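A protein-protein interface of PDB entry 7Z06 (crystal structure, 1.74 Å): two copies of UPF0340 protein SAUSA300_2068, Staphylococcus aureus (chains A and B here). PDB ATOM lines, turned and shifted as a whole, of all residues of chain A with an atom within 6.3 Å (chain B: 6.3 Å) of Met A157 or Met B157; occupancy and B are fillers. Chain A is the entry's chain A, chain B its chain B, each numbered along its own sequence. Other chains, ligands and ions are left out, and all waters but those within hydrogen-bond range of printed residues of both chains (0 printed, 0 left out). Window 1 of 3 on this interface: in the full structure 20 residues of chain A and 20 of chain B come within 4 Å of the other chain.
The guanidinium group (NE) of Arg B96 is in hydrogen-bond range of the backbone carbonyl oxygen (O) of Cys A163, at 2.6 Å.
O of Cys B163 lies within hydrogen-bond range of NE of Arg A96 (2.7 Å).
O of Leu A154 is in hydrogen-bond range of NH1 of Arg A96.
NH2 of Arg A96 is in hydrogen-bond range of O of Thr A153 (2.9 Å).
The side-chain sulfur (SD) of Met A157 sits at hydrogen-bond distance from a ring nitrogen (NE2) of His A158 (3.6 Å).
The side-chain sulfur (SD) of Met B157 sits at hydrogen-bond distance from a ring nitrogen (NE2) of His B158, 3.6 Å away.
NE2 of Gln A89 sits at hydrogen-bond distance from O of Leu A154 (3.3 Å).
NE2 of Gln B89 sits at hydrogen-bond distance from O of Leu B154 (3.3 Å).
Leu A154 touches Cys B163.
O of Gly A156 touches CB of Met B157, 3.5 Å away.
O of Gly B156 touches CB of Met A157 (3.5 Å).
N of Met A157 touches N of Met B157, at 3.5 Å.
CE of Met A157 touches CB of Cys B163 (3.7 Å).
Leu B154 touches Cys A163 (CD1 to SG, 3.8 Å).
CB of Cys A163 touches CE of Met B157, at 3.7 Å.
Met A157 touches three residues of chain B.
Of the printed residues of chain A, Met B157 touches Gly A156 (3.5 Å), Met A157 (3.5 Å) and Cys A163 (3.7 Å).
Of the printed residues of chain B, Gly A156 touches Met B157.
Of the printed residues of chain B, Cys A163 touches Arg B96 (2.6 Å), Leu B154 (3.8 Å) and Met B157 (3.7 Å).
Of the 13 printed residues of chain B, 5 touch a printed residue of chain A.
Hydrophobic or aromatic side chains of chain A that line the printed part of chain B: Leu A154 and Met A157.
Along chain A the printed residues that touch a printed residue of chain B span positions 96 to 163.
Among the printed residues, 9 pairs touch across the chains.
Among the printed residues, no Asp or Glu carboxylate lies within 4 Å of a Lys or Arg side-chain nitrogen of the other chain.
Arg A96 touches Cys B163, and with the chains exchanged Cys A163 touches Arg B96.
Gly A156 touches Met B157, and with the chains exchanged Met A157 touches Gly B156.
Met A157 touches its own counterpart, Met B157.
Met A157 touches Cys B163, and with the chains exchanged Cys A163 touches Met B157.
13 positions are printed for both chains.
Of the 9 pairs that touch across the chains among the printed residues, 9 have their exchanged pair printed and touching as well.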
ATOM      1  N   GLN A  89       7.409   4.104  20.265  1.00  0.00           N
ATOM      2  CA  GLN A  89       8.359   3.117  20.739  1.00  0.00           C
ATOM      3  C   GLN A  89       9.606   3.051  19.852  1.00  0.00           C
ATOM      4  O   GLN A  89       9.508   2.964  18.632  1.00  0.00           O
ATOM      5  CB  GLN A  89       7.723   1.740  20.752  1.00  0.00           C
ATOM      6  CG  GLN A  89       8.621   0.643  21.282  1.00  0.00           C
ATOM      7  CD  GLN A  89       7.980  -0.727  21.195  1.00  0.00           C
ATOM      8  OE1 GLN A  89       7.903  -1.435  22.183  1.00  0.00           O
ATOM      9  NE2 GLN A  89       7.539  -1.125  19.972  1.00  0.00           N
ATOM     10  N   ARG A  96      13.619  -0.326  23.710  1.00  0.00           N
ATOM     11  CA  ARG A  96      12.200   0.058  23.492  1.00  0.00           C
ATOM     12  C   ARG A  96      11.851   1.339  24.256  1.00  0.00           C
ATOM     13  O   ARG A  96      10.693   1.477  24.666  1.00  0.00           O
ATOM     14  CB  ARG A  96      11.276  -1.086  23.926  1.00  0.00           C
ATOM     15  CG  ARG A  96      11.417  -2.348  23.091  1.00  0.00           C
ATOM     16  CD  ARG A  96      10.504  -3.421  23.658  1.00  0.00           C
ATOM     17  NE  ARG A  96      10.556  -4.626  22.869  1.00  0.00           N
ATOM     18  CZ  ARG A  96       9.736  -4.904  21.858  1.00  0.00           C
ATOM     19  NH1 ARG A  96       8.768  -4.070  21.539  1.00  0.00           N
ATOM     20  NH2 ARG A  96       9.898  -6.022  21.175  1.00  0.00           N
ATOM     21  N   ILE A 142       6.457   3.072  29.717  1.00  0.00           N
ATOM     22  CA  ILE A 142       5.229   3.818  29.757  1.00  0.00           C
ATOM     23  C   ILE A 142       4.083   2.825  29.821  1.00  0.00           C
ATOM     24  O   ILE A 142       4.205   1.669  29.362  1.00  0.00           O
ATOM     25  CB  ILE A 142       5.133   4.735  28.488  1.00  0.00           C
ATOM     26  CG1 ILE A 142       4.177   5.922  28.741  1.00  0.00           C
ATOM     27  CG2 ILE A 142       4.731   3.933  27.241  1.00  0.00           C
ATOM     28  CD1 ILE A 142       4.228   6.973  27.658  1.00  0.00           C
ATOM     29  N   THR A 143       2.963   3.293  30.371  1.00  0.00           N
ATOM     30  CA  THR A 143       1.718   2.535  30.400  1.00  0.00           C
ATOM     31  C   THR A 143       0.662   3.442  29.818  1.00  0.00           C
ATOM     32  O   THR A 143       0.397   4.525  30.342  1.00  0.00           O
ATOM     33  CB  THR A 143       1.362   2.130  31.845  1.00  0.00           C
ATOM     34  OG1 THR A 143       2.441   1.346  32.377  1.00  0.00           O
ATOM     35  CG2 THR A 143       0.087   1.301  31.893  1.00  0.00           C
ATOM     36  N   THR A 153       6.308  -5.519  15.909  1.00  0.00           N
ATOM     37  CA  THR A 153       7.402  -5.079  16.792  1.00  0.00           C
ATOM     38  C   THR A 153       7.129  -5.455  18.236  1.00  0.00           C
ATOM     39  O   THR A 153       8.064  -5.508  19.050  1.00  0.00           O
ATOM     40  CB  THR A 153       7.643  -3.550  16.698  1.00  0.00           C
ATOM     41  OG1 THR A 153       6.466  -2.853  17.137  1.00  0.00           O
ATOM     42  CG2 THR A 153       7.985  -3.149  15.268  1.00  0.00           C
ATOM     43  N   LEU A 154       5.842  -5.707  18.544  1.00  0.00           N
ATOM     44  CA  LEU A 154       5.275  -5.992  19.865  1.00  0.00           C
ATOM     45  C   LEU A 154       5.101  -4.725  20.710  1.00  0.00           C
ATOM     46  O   LEU A 154       6.036  -3.926  20.815  1.00  0.00           O
ATOM     47  CB  LEU A 154       6.055  -7.049  20.629  1.00  0.00           C
ATOM     48  CG  LEU A 154       6.311  -8.337  19.844  1.00  0.00           C
ATOM     49  CD1 LEU A 154       6.871  -9.399  20.735  1.00  0.00           C
ATOM     50  CD2 LEU A 154       4.995  -8.786  19.172  1.00  0.00           C
ATOM     51  N   ILE A 155       3.895  -4.535  21.278  1.00  0.00           N
ATOM     52  CA  ILE A 155       3.622  -3.344  22.065  1.00  0.00           C
ATOM     53  C   ILE A 155       2.914  -3.622  23.405  1.00  0.00           C
ATOM     54  O   ILE A 155       2.606  -2.676  24.138  1.00  0.00           O
ATOM     55  CB  ILE A 155       2.788  -2.326  21.275  1.00  0.00           C
ATOM     56  CG1 ILE A 155       1.399  -2.922  20.931  1.00  0.00           C
ATOM     57  CG2 ILE A 155       3.557  -1.851  20.048  1.00  0.00           C
ATOM     58  CD1 ILE A 155       0.471  -1.882  20.395  1.00  0.00           C
ATOM     59  N   GLY A 156       2.669  -4.902  23.706  1.00  0.00           N
ATOM     60  CA  GLY A 156       1.810  -5.286  24.826  1.00  0.00           C
ATOM     61  C   GLY A 156       2.356  -4.929  26.195  1.00  0.00           C
ATOM     62  O   GLY A 156       1.585  -4.735  27.150  1.00  0.00           O
ATOM     63  N   MET A 157       3.693  -4.818  26.286  1.00  0.00           N
ATOM     64  CA  MET A 157       4.371  -4.376  27.491  1.00  0.00           C
ATOM     65  C   MET A 157       4.005  -2.969  27.868  1.00  0.00           C
ATOM     66  O   MET A 157       4.181  -2.573  29.055  1.00  0.00           O
ATOM     67  CB  MET A 157       5.899  -4.540  27.383  1.00  0.00           C
ATOM     68  CG  MET A 157       6.610  -3.661  26.345  1.00  0.00           C
ATOM     69  SD  MET A 157       6.361  -4.072  24.597  1.00  0.00           S
ATOM     70  CE  MET A 157       7.149  -5.653  24.527  1.00  0.00           C
ATOM     71  N   HIS A 158       3.468  -2.190  26.926  1.00  0.00           N
ATOM     72  CA  HIS A 158       3.092  -0.796  27.172  1.00  0.00           C
ATOM     73  C   HIS A 158       1.637  -0.516  27.471  1.00  0.00           C
ATOM     74  O   HIS A 158       1.282   0.618  27.754  1.00  0.00           O
ATOM     75  CB  HIS A 158       3.499   0.068  25.994  1.00  0.00           C
ATOM     76  CG  HIS A 158       4.928  -0.117  25.574  1.00  0.00           C
ATOM     77  ND1 HIS A 158       5.979   0.189  26.404  1.00  0.00           N
ATOM     78  CD2 HIS A 158       5.476  -0.523  24.406  1.00  0.00           C
ATOM     79  CE1 HIS A 158       7.119  -0.038  25.774  1.00  0.00           C
ATOM     80  NE2 HIS A 158       6.840  -0.482  24.555  1.00  0.00           N
ATOM     81  N   ILE A 159       0.783  -1.527  27.315  1.00  0.00           N
ATOM     82  CA  ILE A 159      -0.645  -1.340  27.383  1.00  0.00           C
ATOM     83  C   ILE A 159      -1.121  -1.601  28.825  1.00  0.00           C
ATOM     84  O   ILE A 159      -0.791  -2.600  29.413  1.00  0.00           O
ATOM     85  CB  ILE A 159      -1.386  -2.245  26.383  1.00  0.00           C
ATOM     86  CG1 ILE A 159      -0.806  -2.070  24.939  1.00  0.00           C
ATOM     87  CG2 ILE A 159      -2.873  -1.969  26.431  1.00  0.00           C
ATOM     88  CD1 ILE A 159      -0.936  -0.638  24.446  1.00  0.00           C
ATOM     89  N   HIS A 161      -3.073  -2.863  31.850  1.00  0.00           N
ATOM     90  CA  HIS A 161      -3.783  -4.121  32.111  1.00  0.00           C
ATOM     91  C   HIS A 161      -5.250  -3.779  32.307  1.00  0.00           C
ATOM     92  O   HIS A 161      -5.560  -2.843  33.036  1.00  0.00           O
ATOM     93  CB  HIS A 161      -3.188  -4.754  33.352  1.00  0.00           C
ATOM     94  CG  HIS A 161      -3.599  -6.161  33.591  1.00  0.00           C
ATOM     95  ND1 HIS A 161      -3.317  -7.176  32.702  1.00  0.00           N
ATOM     96  CD2 HIS A 161      -4.225  -6.740  34.641  1.00  0.00           C
ATOM     97  CE1 HIS A 161      -3.731  -8.317  33.198  1.00  0.00           C
ATOM     98  NE2 HIS A 161      -4.288  -8.087  34.376  1.00  0.00           N
ATOM     99  N   CYS A 163      -5.040  -5.736  28.613  1.00  0.00           N
ATOM    100  CA  CYS A 163      -4.883  -5.423  27.203  1.00  0.00           C
ATOM    101  C   CYS A 163      -5.856  -6.283  26.373  1.00  0.00           C
ATOM    102  O   CYS A 163      -5.917  -7.511  26.553  1.00  0.00           O
ATOM    103  CB  CYS A 163      -3.458  -5.721  26.814  1.00  0.00           C
ATOM    104  SG  CYS A 163      -3.091  -5.596  25.039  1.00  0.00           S
ATOM    105  N   GLN B  89      -1.302 -18.511  28.793  1.00  0.00           N
ATOM    106  CA  GLN B  89      -2.083 -17.267  28.997  1.00  0.00           C
ATOM    107  C   GLN B  89      -3.569 -17.518  28.738  1.00  0.00           C
ATOM    108  O   GLN B  89      -3.891 -18.220  27.761  1.00  0.00           O
ATOM    109  CB  GLN B  89      -1.598 -16.166  28.055  1.00  0.00           C
ATOM    110  CG  GLN B  89      -2.290 -14.827  28.256  1.00  0.00           C
ATOM    111  CD  GLN B  89      -1.915 -13.826  27.191  1.00  0.00           C
ATOM    112  OE1 GLN B  89      -1.754 -12.638  27.457  1.00  0.00           O
ATOM    113  NE2 GLN B  89      -1.766 -14.303  25.967  1.00  0.00           N
ATOM    114  N   ARG B  96      -6.349 -12.281  31.286  1.00  0.00           N
ATOM    115  CA  ARG B  96      -5.050 -12.813  30.800  1.00  0.00           C
ATOM    116  C   ARG B  96      -4.322 -13.510  31.952  1.00  0.00           C
ATOM    117  O   ARG B  96      -3.082 -13.560  31.918  1.00  0.00           O
ATOM    118  CB  ARG B  96      -4.202 -11.689  30.199  1.00  0.00           C
ATOM    119  CG  ARG B  96      -4.748 -11.112  28.901  1.00  0.00           C
ATOM    120  CD  ARG B  96      -3.861  -9.988  28.398  1.00  0.00           C
ATOM    121  NE  ARG B  96      -4.317  -9.409  27.144  1.00  0.00           N
ATOM    122  CZ  ARG B  96      -3.886  -9.776  25.943  1.00  0.00           C
ATOM    123  NH1 ARG B  96      -2.978 -10.730  25.828  1.00  0.00           N
ATOM    124  NH2 ARG B  96      -4.363  -9.186  24.863  1.00  0.00           N
ATOM    125  N   ILE B 142       2.786 -12.699  35.186  1.00  0.00           N
ATOM    126  CA  ILE B 142       4.004 -13.462  35.182  1.00  0.00           C
ATOM    127  C   ILE B 142       5.014 -12.710  34.308  1.00  0.00           C
ATOM    128  O   ILE B 142       4.632 -11.975  33.386  1.00  0.00           O
ATOM    129  CB  ILE B 142       3.750 -14.915  34.669  1.00  0.00           C
ATOM    130  CG1 ILE B 142       4.833 -15.884  35.162  1.00  0.00           C
ATOM    131  CG2 ILE B 142       3.601 -14.940  33.165  1.00  0.00           C
ATOM    132  CD1 ILE B 142       4.507 -17.356  34.900  1.00  0.00           C
ATOM    133  N   THR B 143       6.286 -12.919  34.606  1.00  0.00           N
ATOM    134  CA  THR B 143       7.397 -12.413  33.788  1.00  0.00           C
ATOM    135  C   THR B 143       8.276 -13.579  33.466  1.00  0.00           C
ATOM    136  O   THR B 143       8.797 -14.231  34.365  1.00  0.00           O
ATOM    137  CB  THR B 143       8.176 -11.306  34.525  1.00  0.00           C
ATOM    138  OG1 THR B 143       7.275 -10.240  34.816  1.00  0.00           O
ATOM    139  CG2 THR B 143       9.305 -10.733  33.678  1.00  0.00           C
ATOM    140  N   THR B 153      -2.721 -12.813  19.928  1.00  0.00           N
ATOM    141  CA  THR B 153      -3.389 -12.569  21.213  1.00  0.00           C
ATOM    142  C   THR B 153      -2.635 -11.501  22.023  1.00  0.00           C
ATOM    143  O   THR B 153      -3.221 -10.913  22.951  1.00  0.00           O
ATOM    144  CB  THR B 153      -3.506 -13.851  22.064  1.00  0.00           C
ATOM    145  OG1 THR B 153      -2.201 -14.357  22.378  1.00  0.00           O
ATOM    146  CG2 THR B 153      -4.292 -14.861  21.385  1.00  0.00           C
ATOM    147  N   LEU B 154      -1.363 -11.298  21.675  1.00  0.00           N
ATOM    148  CA  LEU B 154      -0.382 -10.436  22.366  1.00  0.00           C
ATOM    149  C   LEU B 154       0.176 -11.086  23.621  1.00  0.00           C
ATOM    150  O   LEU B 154      -0.586 -11.579  24.467  1.00  0.00           O
ATOM    151  CB  LEU B 154      -0.955  -9.040  22.681  1.00  0.00           C
ATOM    152  CG  LEU B 154      -1.530  -8.295  21.500  1.00  0.00           C
ATOM    153  CD1 LEU B 154      -1.528  -6.820  21.826  1.00  0.00           C
ATOM    154  CD2 LEU B 154      -0.639  -8.472  20.236  1.00  0.00           C
ATOM    155  N   ILE B 155       1.510 -11.089  23.748  1.00  0.00           N
ATOM    156  CA  ILE B 155       2.171 -11.682  24.890  1.00  0.00           C
ATOM    157  C   ILE B 155       3.267 -10.816  25.521  1.00  0.00           C
ATOM    158  O   ILE B 155       3.884 -11.238  26.483  1.00  0.00           O
ATOM    159  CB  ILE B 155       2.762 -13.051  24.569  1.00  0.00           C
ATOM    160  CG1 ILE B 155       3.874 -12.917  23.477  1.00  0.00           C
ATOM    161  CG2 ILE B 155       1.652 -14.022  24.136  1.00  0.00           C
ATOM    162  CD1 ILE B 155       4.633 -14.216  23.315  1.00  0.00           C
ATOM    163  N   GLY B 156       3.450  -9.609  24.991  1.00  0.00           N
ATOM    164  CA  GLY B 156       4.552  -8.740  25.332  1.00  0.00           C
ATOM    165  C   GLY B 156       4.587  -8.278  26.781  1.00  0.00           C
ATOM    166  O   GLY B 156       5.673  -8.025  27.343  1.00  0.00           O
ATOM    167  N   MET B 157       3.405  -8.184  27.367  1.00  0.00           N
ATOM    168  CA  MET B 157       3.237  -7.827  28.771  1.00  0.00           C
ATOM    169  C   MET B 157       3.850  -8.856  29.693  1.00  0.00           C
ATOM    170  O   MET B 157       4.131  -8.541  30.859  1.00  0.00           O
ATOM    171  CB  MET B 157       1.751  -7.579  29.108  1.00  0.00           C
ATOM    172  CG  MET B 157       0.826  -8.802  29.045  1.00  0.00           C
ATOM    173  SD  MET B 157       0.374  -9.406  27.378  1.00  0.00           S
ATOM    174  CE  MET B 157      -0.537  -8.011  26.770  1.00  0.00           C
ATOM    175  N   HIS B 158       4.086 -10.072  29.199  1.00  0.00           N
ATOM    176  CA  HIS B 158       4.658 -11.152  30.009  1.00  0.00           C
ATOM    177  C   HIS B 158       6.151 -11.401  29.875  1.00  0.00           C
ATOM    178  O   HIS B 158       6.698 -12.245  30.574  1.00  0.00           O
ATOM    179  CB  HIS B 158       3.951 -12.468  29.714  1.00  0.00           C
ATOM    180  CG  HIS B 158       2.461 -12.378  29.772  1.00  0.00           C
ATOM    181  ND1 HIS B 158       1.795 -12.069  30.943  1.00  0.00           N
ATOM    182  CD2 HIS B 158       1.508 -12.588  28.832  1.00  0.00           C
ATOM    183  CE1 HIS B 158       0.493 -12.101  30.720  1.00  0.00           C
ATOM    184  NE2 HIS B 158       0.285 -12.387  29.448  1.00  0.00           N
ATOM    185  N   ILE B 159       6.790 -10.732  28.908  1.00  0.00           N
ATOM    186  CA  ILE B 159       8.149 -11.017  28.560  1.00  0.00           C
ATOM    187  C   ILE B 159       9.071 -10.069  29.342  1.00  0.00           C
ATOM    188  O   ILE B 159       8.857  -8.875  29.358  1.00  0.00           O
ATOM    189  CB  ILE B 159       8.399 -10.881  27.042  1.00  0.00           C
ATOM    190  CG1 ILE B 159       7.385 -11.745  26.241  1.00  0.00           C
ATOM    191  CG2 ILE B 159       9.838 -11.256  26.726  1.00  0.00           C
ATOM    192  CD1 ILE B 159       7.494 -13.216  26.591  1.00  0.00           C
ATOM    193  N   HIS B 161      11.785  -7.582  30.290  1.00  0.00           N
ATOM    194  CA  HIS B 161      12.412  -6.461  29.579  1.00  0.00           C
ATOM    195  C   HIS B 161      13.893  -6.794  29.418  1.00  0.00           C
ATOM    196  O   HIS B 161      14.513  -7.234  30.380  1.00  0.00           O
ATOM    197  CB  HIS B 161      12.228  -5.194  30.405  1.00  0.00           C
ATOM    198  CG  HIS B 161      12.547  -3.938  29.673  1.00  0.00           C
ATOM    199  ND1 HIS B 161      11.876  -3.544  28.538  1.00  0.00           N
ATOM    200  CD2 HIS B 161      13.419  -2.942  29.965  1.00  0.00           C
ATOM    201  CE1 HIS B 161      12.313  -2.355  28.167  1.00  0.00           C
ATOM    202  NE2 HIS B 161      13.255  -1.968  29.010  1.00  0.00           N
ATOM    203  N   CYS B 163      12.180  -7.121  25.622  1.00  0.00           N
ATOM    204  CA  CYS B 163      11.590  -8.142  24.754  1.00  0.00           C
ATOM    205  C   CYS B 163      12.121  -7.971  23.334  1.00  0.00           C
ATOM    206  O   CYS B 163      12.098  -6.852  22.797  1.00  0.00           O
ATOM    207  CB  CYS B 163      10.097  -7.951  24.815  1.00  0.00           C
ATOM    208  SG  CYS B 163       9.186  -9.009  23.662  1.00  0.00           S
